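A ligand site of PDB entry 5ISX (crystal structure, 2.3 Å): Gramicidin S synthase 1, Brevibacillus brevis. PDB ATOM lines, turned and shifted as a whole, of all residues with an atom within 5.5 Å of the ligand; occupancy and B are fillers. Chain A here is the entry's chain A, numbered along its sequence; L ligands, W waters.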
ATOM      1  N   ASP A  36      -7.453   7.597   0.859  1.00  0.00           N
ATOM      2  CA  ASP A  36      -7.201   8.893   1.476  1.00  0.00           C
ATOM      3  C   ASP A  36      -8.539   9.508   1.893  1.00  0.00           C
ATOM      4  O   ASP A  36      -9.590   8.879   1.737  1.00  0.00           O
ATOM      5  CB  ASP A  36      -6.429   9.837   0.537  1.00  0.00           C
ATOM      6  CG  ASP A  36      -7.158  10.081  -0.787  1.00  0.00           C
ATOM      7  OD1 ASP A  36      -8.394  10.241  -0.801  1.00  0.00           O
ATOM      8  OD2 ASP A  36      -6.467  10.122  -1.833  1.00  0.00           O
ATOM      9  N   SER A  37      -8.511  10.743   2.387  1.00  0.00           N
ATOM     10  CA  SER A  37      -9.722  11.368   2.905  1.00  0.00           C
ATOM     11  C   SER A  37     -10.709  11.761   1.811  1.00  0.00           C
ATOM     12  O   SER A  37     -11.893  11.965   2.081  1.00  0.00           O
ATOM     13  CB  SER A  37      -9.375  12.598   3.733  1.00  0.00           C
ATOM     14  N   ILE A  38     -10.243  11.854   0.568  1.00  0.00           N
ATOM     15  CA  ILE A  38     -11.144  12.102  -0.570  1.00  0.00           C
ATOM     16  C   ILE A  38     -11.854  10.807  -0.980  1.00  0.00           C
ATOM     17  O   ILE A  38     -13.052  10.804  -1.225  1.00  0.00           O
ATOM     18  CB  ILE A  38     -10.389  12.721  -1.776  1.00  0.00           C
ATOM     19  CG1 ILE A  38      -9.998  14.164  -1.457  1.00  0.00           C
ATOM     20  CG2 ILE A  38     -11.264  12.670  -3.031  1.00  0.00           C
ATOM     21  CD1 ILE A  38      -9.288  14.880  -2.597  1.00  0.00           C
ATOM     22  N   GLN A 110     -12.003  26.047 -14.091  1.00  0.00           N
ATOM     23  CA  GLN A 110     -11.391  24.733 -14.188  1.00  0.00           C
ATOM     24  C   GLN A 110     -11.923  24.088 -15.454  1.00  0.00           C
ATOM     25  O   GLN A 110     -12.972  24.466 -15.963  1.00  0.00           O
ATOM     26  CB  GLN A 110     -11.692  23.881 -12.952  1.00  0.00           C
ATOM     27  CG  GLN A 110     -10.910  24.296 -11.717  1.00  0.00           C
ATOM     28  CD  GLN A 110     -11.090  23.326 -10.567  1.00  0.00           C
ATOM     29  OE1 GLN A 110     -12.208  22.851 -10.303  1.00  0.00           O
ATOM     30  NE2 GLN A 110     -10.009  23.022  -9.869  1.00  0.00           N
ATOM     31  N   HIS A 217     -14.847  28.558 -11.716  1.00  0.00           N
ATOM     32  CA  HIS A 217     -14.456  27.971 -10.449  1.00  0.00           C
ATOM     33  C   HIS A 217     -15.442  28.256  -9.320  1.00  0.00           C
ATOM     34  O   HIS A 217     -15.469  27.528  -8.336  1.00  0.00           O
ATOM     35  CB  HIS A 217     -13.056  28.441 -10.032  1.00  0.00           C
ATOM     36  CG  HIS A 217     -12.279  27.400  -9.300  1.00  0.00           C
ATOM     37  ND1 HIS A 217     -12.869  26.452  -8.499  1.00  0.00           N
ATOM     38  CD2 HIS A 217     -10.946  27.137  -9.271  1.00  0.00           C
ATOM     39  CE1 HIS A 217     -11.954  25.657  -7.988  1.00  0.00           C
ATOM     40  NE2 HIS A 217     -10.771  26.048  -8.443  1.00  0.00           N
ATOM     41  N   ASP A 221     -15.226  22.224  -7.993  1.00  0.00           N
ATOM     42  CA  ASP A 221     -13.890  21.911  -7.468  1.00  0.00           C
ATOM     43  C   ASP A 221     -13.541  20.455  -7.805  1.00  0.00           C
ATOM     44  O   ASP A 221     -14.335  19.760  -8.428  1.00  0.00           O
ATOM     45  CB  ASP A 221     -13.791  22.164  -5.953  1.00  0.00           C
ATOM     46  CG  ASP A 221     -14.771  21.340  -5.127  1.00  0.00           C
ATOM     47  OD1 ASP A 221     -15.381  20.376  -5.650  1.00  0.00           O
ATOM     48  OD2 ASP A 221     -14.923  21.637  -3.921  1.00  0.00           O
ATOM     49  N   GLY A 222     -12.362  20.020  -7.382  1.00  0.00           N
ATOM     50  CA  GLY A 222     -11.852  18.692  -7.704  1.00  0.00           C
ATOM     51  C   GLY A 222     -12.766  17.509  -7.435  1.00  0.00           C
ATOM     52  O   GLY A 222     -12.881  16.614  -8.267  1.00  0.00           O
ATOM     53  N   ILE A 223     -13.414  17.503  -6.275  1.00  0.00           N
ATOM     54  CA  ILE A 223     -14.377  16.463  -5.937  1.00  0.00           C
ATOM     55  C   ILE A 223     -15.650  16.588  -6.786  1.00  0.00           C
ATOM     56  O   ILE A 223     -16.212  15.591  -7.238  1.00  0.00           O
ATOM     57  CB  ILE A 223     -14.733  16.495  -4.423  1.00  0.00           C
ATOM     58  CG1 ILE A 223     -13.488  16.199  -3.584  1.00  0.00           C
ATOM     59  CG2 ILE A 223     -15.854  15.506  -4.096  1.00  0.00           C
ATOM     60  CD1 ILE A 223     -13.742  16.031  -2.104  1.00  0.00           C
ATOM     61  N   GLU A 329      -0.860  10.494   7.238  1.00  0.00           N
ATOM     62  CA  GLU A 329      -1.626  10.678   6.008  1.00  0.00           C
ATOM     63  C   GLU A 329      -0.709  11.375   5.000  1.00  0.00           C
ATOM     64  O   GLU A 329       0.297  11.966   5.400  1.00  0.00           O
ATOM     65  CB  GLU A 329      -2.888  11.497   6.255  1.00  0.00           C
ATOM     66  CG  GLU A 329      -3.825  10.891   7.278  1.00  0.00           C
ATOM     67  CD  GLU A 329      -4.845  11.890   7.792  1.00  0.00           C
ATOM     68  OE1 GLU A 329      -4.639  13.109   7.601  1.00  0.00           O
ATOM     69  OE2 GLU A 329      -5.855  11.456   8.377  1.00  0.00           O
ATOM     70  N   ILE A 330      -1.044  11.306   3.719  1.00  0.00           N
ATOM     71  CA  ILE A 330      -0.126  11.758   2.677  1.00  0.00           C
ATOM     72  C   ILE A 330       0.305  13.232   2.840  1.00  0.00           C
ATOM     73  O   ILE A 330       1.444  13.575   2.508  1.00  0.00           O
ATOM     74  CB  ILE A 330      -0.726  11.555   1.261  1.00  0.00           C
ATOM     75  CG1 ILE A 330       0.324  11.818   0.182  1.00  0.00           C
ATOM     76  CG2 ILE A 330      -1.961  12.402   1.047  1.00  0.00           C
ATOM     77  CD1 ILE A 330      -0.086  11.383  -1.201  1.00  0.00           C
ATOM     78  N   ASN A 331      -0.573  14.082   3.362  1.00  0.00           N
ATOM     79  CA  ASN A 331      -0.190  15.464   3.681  1.00  0.00           C
ATOM     80  C   ASN A 331       1.042  15.553   4.577  1.00  0.00           C
ATOM     81  O   ASN A 331       1.916  16.396   4.366  1.00  0.00           O
ATOM     82  CB  ASN A 331      -1.337  16.206   4.346  1.00  0.00           C
ATOM     83  CG  ASN A 331      -2.248  16.894   3.353  1.00  0.00           C
ATOM     84  OD1 ASN A 331      -2.134  16.690   2.149  1.00  0.00           O
ATOM     85  ND2 ASN A 331      -3.167  17.712   3.861  1.00  0.00           N
ATOM     86  N   GLU A 356      -4.180  24.143   0.872  1.00  0.00           N
ATOM     87  CA  GLU A 356      -5.554  23.924   0.430  1.00  0.00           C
ATOM     88  C   GLU A 356      -6.050  22.534   0.843  1.00  0.00           C
ATOM     89  O   GLU A 356      -5.283  21.576   0.833  1.00  0.00           O
ATOM     90  CB  GLU A 356      -5.677  24.098  -1.081  1.00  0.00           C
ATOM     91  CG  GLU A 356      -5.175  25.453  -1.577  1.00  0.00           C
ATOM     92  CD  GLU A 356      -5.503  25.708  -3.025  1.00  0.00           C
ATOM     93  OE1 GLU A 356      -4.739  26.449  -3.680  1.00  0.00           O
ATOM     94  OE2 GLU A 356      -6.528  25.190  -3.508  1.00  0.00           O
ATOM     95  N   GLY A 357      -7.319  22.464   1.232  1.00  0.00           N
ATOM     96  CA  GLY A 357      -7.973  21.194   1.548  1.00  0.00           C
ATOM     97  C   GLY A 357      -9.299  21.100   0.825  1.00  0.00           C
ATOM     98  O   GLY A 357      -9.802  22.120   0.341  1.00  0.00           O
ATOM     99  N   HIS A 358      -9.884  19.915   0.749  1.00  0.00           N
ATOM    100  CA  HIS A 358     -11.148  19.761   0.026  1.00  0.00           C
ATOM    101  C   HIS A 358     -12.271  20.518   0.737  1.00  0.00           C
ATOM    102  O   HIS A 358     -13.273  20.874   0.120  1.00  0.00           O
ATOM    103  CB  HIS A 358     -11.517  18.280  -0.163  1.00  0.00           C
ATOM    104  CG  HIS A 358     -11.508  17.487   1.109  1.00  0.00           C
ATOM    105  ND1 HIS A 358     -12.513  17.589   2.057  1.00  0.00           N
ATOM    106  CD2 HIS A 358     -10.629  16.584   1.598  1.00  0.00           C
ATOM    107  CE1 HIS A 358     -12.234  16.783   3.070  1.00  0.00           C
ATOM    108  NE2 HIS A 358     -11.108  16.161   2.809  1.00  0.00           N
ATOM    109  N   GLY A 359     -12.091  20.753   2.032  1.00  0.00           N
ATOM    110  CA  GLY A 359     -13.001  21.580   2.795  1.00  0.00           C
ATOM    111  C   GLY A 359     -14.320  20.945   3.185  1.00  0.00           C
ATOM    112  O   GLY A 359     -15.175  21.604   3.774  1.00  0.00           O
ATOM    113  N   GLU A 361     -15.494  19.053   5.614  1.00  0.00           N
ATOM    114  CA  GLU A 361     -15.325  18.509   6.948  1.00  0.00           C
ATOM    115  C   GLU A 361     -16.659  18.350   7.651  1.00  0.00           C
ATOM    116  O   GLU A 361     -17.542  19.197   7.518  1.00  0.00           O
ATOM    117  CB  GLU A 361     -14.393  19.390   7.783  1.00  0.00           C
ATOM    118  CG  GLU A 361     -13.042  19.577   7.168  1.00  0.00           C
ATOM    119  CD  GLU A 361     -12.331  18.255   6.927  1.00  0.00           C
ATOM    120  OE1 GLU A 361     -12.434  17.367   7.791  1.00  0.00           O
ATOM    121  OE2 GLU A 361     -11.694  18.106   5.869  1.00  0.00           O
ATOM    122  N   TRP A 375     -17.974  24.865  -4.947  1.00  0.00           N
ATOM    123  CA  TRP A 375     -16.603  25.224  -4.603  1.00  0.00           C
ATOM    124  C   TRP A 375     -16.422  25.162  -3.087  1.00  0.00           C
ATOM    125  O   TRP A 375     -16.694  26.135  -2.390  1.00  0.00           O
ATOM    126  CB  TRP A 375     -16.267  26.621  -5.123  1.00  0.00           C
ATOM    127  CG  TRP A 375     -14.794  26.893  -5.172  1.00  0.00           C
ATOM    128  CD1 TRP A 375     -13.782  26.017  -4.906  1.00  0.00           C
ATOM    129  CD2 TRP A 375     -14.163  28.138  -5.513  1.00  0.00           C
ATOM    130  NE1 TRP A 375     -12.569  26.632  -5.048  1.00  0.00           N
ATOM    131  CE2 TRP A 375     -12.769  27.939  -5.424  1.00  0.00           C
ATOM    132  CE3 TRP A 375     -14.637  29.404  -5.873  1.00  0.00           C
ATOM    133  CZ2 TRP A 375     -11.845  28.947  -5.692  1.00  0.00           C
ATOM    134  CZ3 TRP A 375     -13.720  30.405  -6.139  1.00  0.00           C
ATOM    135  CH2 TRP A 375     -12.337  30.174  -6.047  1.00  0.00           C
ATOM    136  N   THR A 377     -13.508  24.164  -1.489  1.00  0.00           N
ATOM    137  CA  THR A 377     -12.096  24.278  -1.125  1.00  0.00           C
ATOM    138  C   THR A 377     -11.834  25.184   0.077  1.00  0.00           C
ATOM    139  O   THR A 377     -12.312  26.321   0.143  1.00  0.00           O
ATOM    140  CB  THR A 377     -11.277  24.813  -2.308  1.00  0.00           C
ATOM    141  OG1 THR A 377     -11.462  23.957  -3.444  1.00  0.00           O
ATOM    142  CG2 THR A 377      -9.792  24.840  -1.957  1.00  0.00           C
ATOM    143  N   LYS A 409      -9.233  20.288  10.333  1.00  0.00           N
ATOM    144  CA  LYS A 409      -8.525  20.439   9.069  1.00  0.00           C
ATOM    145  C   LYS A 409      -8.397  21.905   8.604  1.00  0.00           C
ATOM    146  O   LYS A 409      -8.380  22.172   7.408  1.00  0.00           O
ATOM    147  CB  LYS A 409      -9.212  19.611   7.977  1.00  0.00           C
ATOM    148  CG  LYS A 409      -9.154  18.105   8.207  1.00  0.00           C
ATOM    149  CD  LYS A 409      -7.801  17.547   7.798  1.00  0.00           C
ATOM    150  CE  LYS A 409      -7.789  16.025   7.855  1.00  0.00           C
ATOM    151  NZ  LYS A 409      -6.495  15.466   7.366  1.00  0.00           N
ATOM    152  N   ASN A 439      -1.079  22.631  -2.927  1.00  0.00           N
ATOM    153  CA  ASN A 439      -2.373  22.127  -3.365  1.00  0.00           C
ATOM    154  C   ASN A 439      -2.276  20.757  -4.014  1.00  0.00           C
ATOM    155  O   ASN A 439      -2.115  20.644  -5.232  1.00  0.00           O
ATOM    156  CB  ASN A 439      -3.019  23.123  -4.333  1.00  0.00           C
ATOM    157  CG  ASN A 439      -4.419  22.724  -4.749  1.00  0.00           C
ATOM    158  OD1 ASN A 439      -5.069  21.919  -4.084  1.00  0.00           O
ATOM    159  ND2 ASN A 439      -4.897  23.302  -5.836  1.00  0.00           N
ATOM    160  N   TYR A 440      -2.362  19.703  -3.208  1.00  0.00           N
ATOM    161  CA  TYR A 440      -2.358  18.348  -3.729  1.00  0.00           C
ATOM    162  C   TYR A 440      -3.801  17.872  -3.956  1.00  0.00           C
ATOM    163  O   TYR A 440      -4.576  17.713  -2.998  1.00  0.00           O
ATOM    164  CB  TYR A 440      -1.595  17.403  -2.784  1.00  0.00           C
ATOM    165  CG  TYR A 440      -1.795  15.946  -3.098  1.00  0.00           C
ATOM    166  CD1 TYR A 440      -1.405  15.417  -4.326  1.00  0.00           C
ATOM    167  CD2 TYR A 440      -2.396  15.100  -2.170  1.00  0.00           C
ATOM    168  CE1 TYR A 440      -1.603  14.074  -4.616  1.00  0.00           C
ATOM    169  CE2 TYR A 440      -2.594  13.757  -2.460  1.00  0.00           C
ATOM    170  CZ  TYR A 440      -2.199  13.253  -3.676  1.00  0.00           C
ATOM    171  OH  TYR A 440      -2.402  11.916  -3.959  1.00  0.00           O
ATOM    172  N   LEU A 441      -4.141  17.644  -5.215  1.00  0.00           N
ATOM    173  CA  LEU A 441      -5.523  17.396  -5.626  1.00  0.00           C
ATOM    174  C   LEU A 441      -5.988  15.957  -5.397  1.00  0.00           C
ATOM    175  O   LEU A 441      -7.185  15.687  -5.416  1.00  0.00           O
ATOM    176  CB  LEU A 441      -5.698  17.750  -7.113  1.00  0.00           C
ATOM    177  CG  LEU A 441      -5.587  19.249  -7.414  1.00  0.00           C
ATOM    178  CD1 LEU A 441      -5.740  19.554  -8.905  1.00  0.00           C
ATOM    179  CD2 LEU A 441      -6.613  20.015  -6.606  1.00  0.00           C
ATOM    180  N   GLY A 442      -5.038  15.047  -5.185  1.00  0.00           N
ATOM    181  CA  GLY A 442      -5.366  13.659  -4.952  1.00  0.00           C
ATOM    182  C   GLY A 442      -5.341  12.767  -6.183  1.00  0.00           C
ATOM    183  O   GLY A 442      -4.665  13.069  -7.173  1.00  0.00           O
ATOM    184  N   LEU A 464      -7.126  21.007 -14.121  1.00  0.00           N
ATOM    185  CA  LEU A 464      -7.795  21.347 -12.863  1.00  0.00           C
ATOM    186  C   LEU A 464      -6.993  22.326 -12.018  1.00  0.00           C
ATOM    187  O   LEU A 464      -7.430  22.746 -10.947  1.00  0.00           O
ATOM    188  CB  LEU A 464      -8.099  20.085 -12.045  1.00  0.00           C
ATOM    189  CG  LEU A 464      -9.145  19.146 -12.650  1.00  0.00           C
ATOM    190  CD1 LEU A 464      -9.469  17.995 -11.719  1.00  0.00           C
ATOM    191  CD2 LEU A 464     -10.405  19.916 -13.033  1.00  0.00           C
HETATM  192  O1  LIG L   1      -6.191  13.759   3.982  1.00  0.00           O
HETATM  193  P1  LIG L   1      -7.451  14.408   3.468  1.00  0.00           P
HETATM  194  O2  LIG L   1      -8.140  15.136   4.605  1.00  0.00           O
HETATM  195  O3  LIG L   1      -8.386  13.349   2.942  1.00  0.00           O
HETATM  196  O4  LIG L   1      -7.108  15.456   2.302  1.00  0.00           O
HETATM  197  C1  LIG L   1      -7.042  14.966   0.966  1.00  0.00           C
HETATM  198  C2  LIG L   1      -5.744  15.518   0.314  1.00  0.00           C
HETATM  199  C3  LIG L   1      -4.558  14.751   0.861  1.00  0.00           C
HETATM  200  C4  LIG L   1      -5.842  15.307  -1.190  1.00  0.00           C
HETATM  201  C5  LIG L   1      -5.546  16.993   0.642  1.00  0.00           C
HETATM  202  O5  LIG L   1      -4.295  17.413   0.164  1.00  0.00           O
HETATM  203  C6  LIG L   1      -6.680  17.845   0.061  1.00  0.00           C
HETATM  204  O6  LIG L   1      -7.712  17.971   0.702  1.00  0.00           O
HETATM  205  N1  LIG L   1      -6.549  18.529  -1.222  1.00  0.00           N
HETATM  206  C7  LIG L   1      -7.674  19.308  -1.697  1.00  0.00           C
HETATM  207  C8  LIG L   1      -7.333  20.364  -2.756  1.00  0.00           C
HETATM  208  C9  LIG L   1      -8.583  20.655  -3.565  1.00  0.00           C
HETATM  209  O7  LIG L   1      -9.593  20.038  -3.291  1.00  0.00           O
HETATM  210  N2  LIG L   1      -8.615  21.618  -4.645  1.00  0.00           N
HETATM  211  C10 LIG L   1      -9.865  21.807  -5.330  1.00  0.00           C
HETATM  212  C11 LIG L   1      -9.765  22.683  -6.571  1.00  0.00           C
HETATM  213  S1  LIG L   1      -9.359  24.355  -6.139  1.00  0.00           S
HETATM  214  O   HOH W   1      -7.945  17.953   3.571  1.00  0.00           O
HETATM  215  O   HOH W   2      -5.196  19.624   2.885  1.00  0.00           O
HETATM  216  O   HOH W   3     -12.330  19.346  -4.054  1.00  0.00           O
HETATM  217  O   HOH W   4      -3.160  20.107  -0.532  1.00  0.00           O
HETATM  218  O   HOH W   5      -3.769  14.020   4.173  1.00  0.00           O
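The backbone NH (N) of Ser 37 sits close to an oxygen (O3) of the ligand (2.7 Å). A side-chain carbon (CB) of Ser 37 is covalently linked to an oxygen (O3) of the ligand (1.5 Å). The backbone carbonyl oxygen (O) of Tyr 440 sits at hydrogen-bond distance from a nitrogen (N1) of the ligand (2.8 Å). O6 of the ligand sits at hydrogen-bond distance from N of His 358 (2.9 Å). OD1 of Asn 331 sits at hydrogen-bond distance from O5 of the ligand, at 3.0 Å. S1 of the ligand sits close to NE2 of His 217, at 3.2 Å. O2 of the ligand sits at hydrogen-bond distance from NZ of Lys 409 (3.2 Å). OG1 of Thr 377 sits close to S1 of the ligand (3.4 Å). An oxygen (O3) of the ligand lies within hydrogen-bond range of the backbone NH of Ile 38 (3.4 Å).
ND2 of Asn 439 is in hydrogen-bond range of OE2 of Glu 356 (3.4 Å). NE2 of Gln 110 is in hydrogen-bond range of NE2 of His 217, at 3.4 Å. A ring nitrogen (ND1) of His 217 sits close to the indole nitrogen of Trp 375, 3.5 Å away. NZ of Lys 409 lies within salt-bridge range of OE1 of Glu 329. NE1 of Trp 375 sits at hydrogen-bond distance from OG1 of Thr 377, at 3.3 Å. The side-chain amide nitrogen (NE2) of Gln 110 lies within hydrogen-bond range of the backbone carbonyl oxygen (O) of Leu 464 (2.8 Å). The backbone NH (N) of Ile 38 is in hydrogen-bond range of the side-chain carboxylate (OD1) of Asp 36 (2.8 Å).
Residues that only touch the ligand: Asp 36, Gln 110, Asp 221, Gly 222, Glu 329, Ile 330, Glu 356, Gly 357, Asn 439 and Leu 441. Hydrophobic or aromatic side chains that line the ligand: Ile 38, His 217, Ile 330, His 358, Tyr 440 and Leu 441. 18 residues have an atom within 4 Å of the ligand: Asp 36, Ser 37, Ile 38, Gln 110, His 217, Asp 221, Gly 222, Glu 329, Ile 330, Asn 331, Glu 356, Gly 357, His 358, Thr 377, Lys 409, Asn 439, Tyr 440 and Leu 441. The nearest printed residue that does not touch the ligand is Gly 442 (4.1 Å).
Water W5 bridges an oxygen (O1) of the ligand (2.4 Å) and the backbone NH of Asn 331 (3.3 Å). Water W3 lies within hydrogen-bond range of O7 of the ligand (2.9 Å), N of Ile 223 (3.1 Å), N of Gly 222 (3.4 Å) and OD2 of Asp 221 (3.5 Å). Water W4 lies within hydrogen-bond range of the backbone NH of Tyr 440, the backbone carbonyl oxygen of Glu 356 and an oxygen (O5) of the ligand. Water W2 bridges the backbone carbonyl oxygen (O) of Glu 356 and the side-chain amide nitrogen (ND2) of Asn 331.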
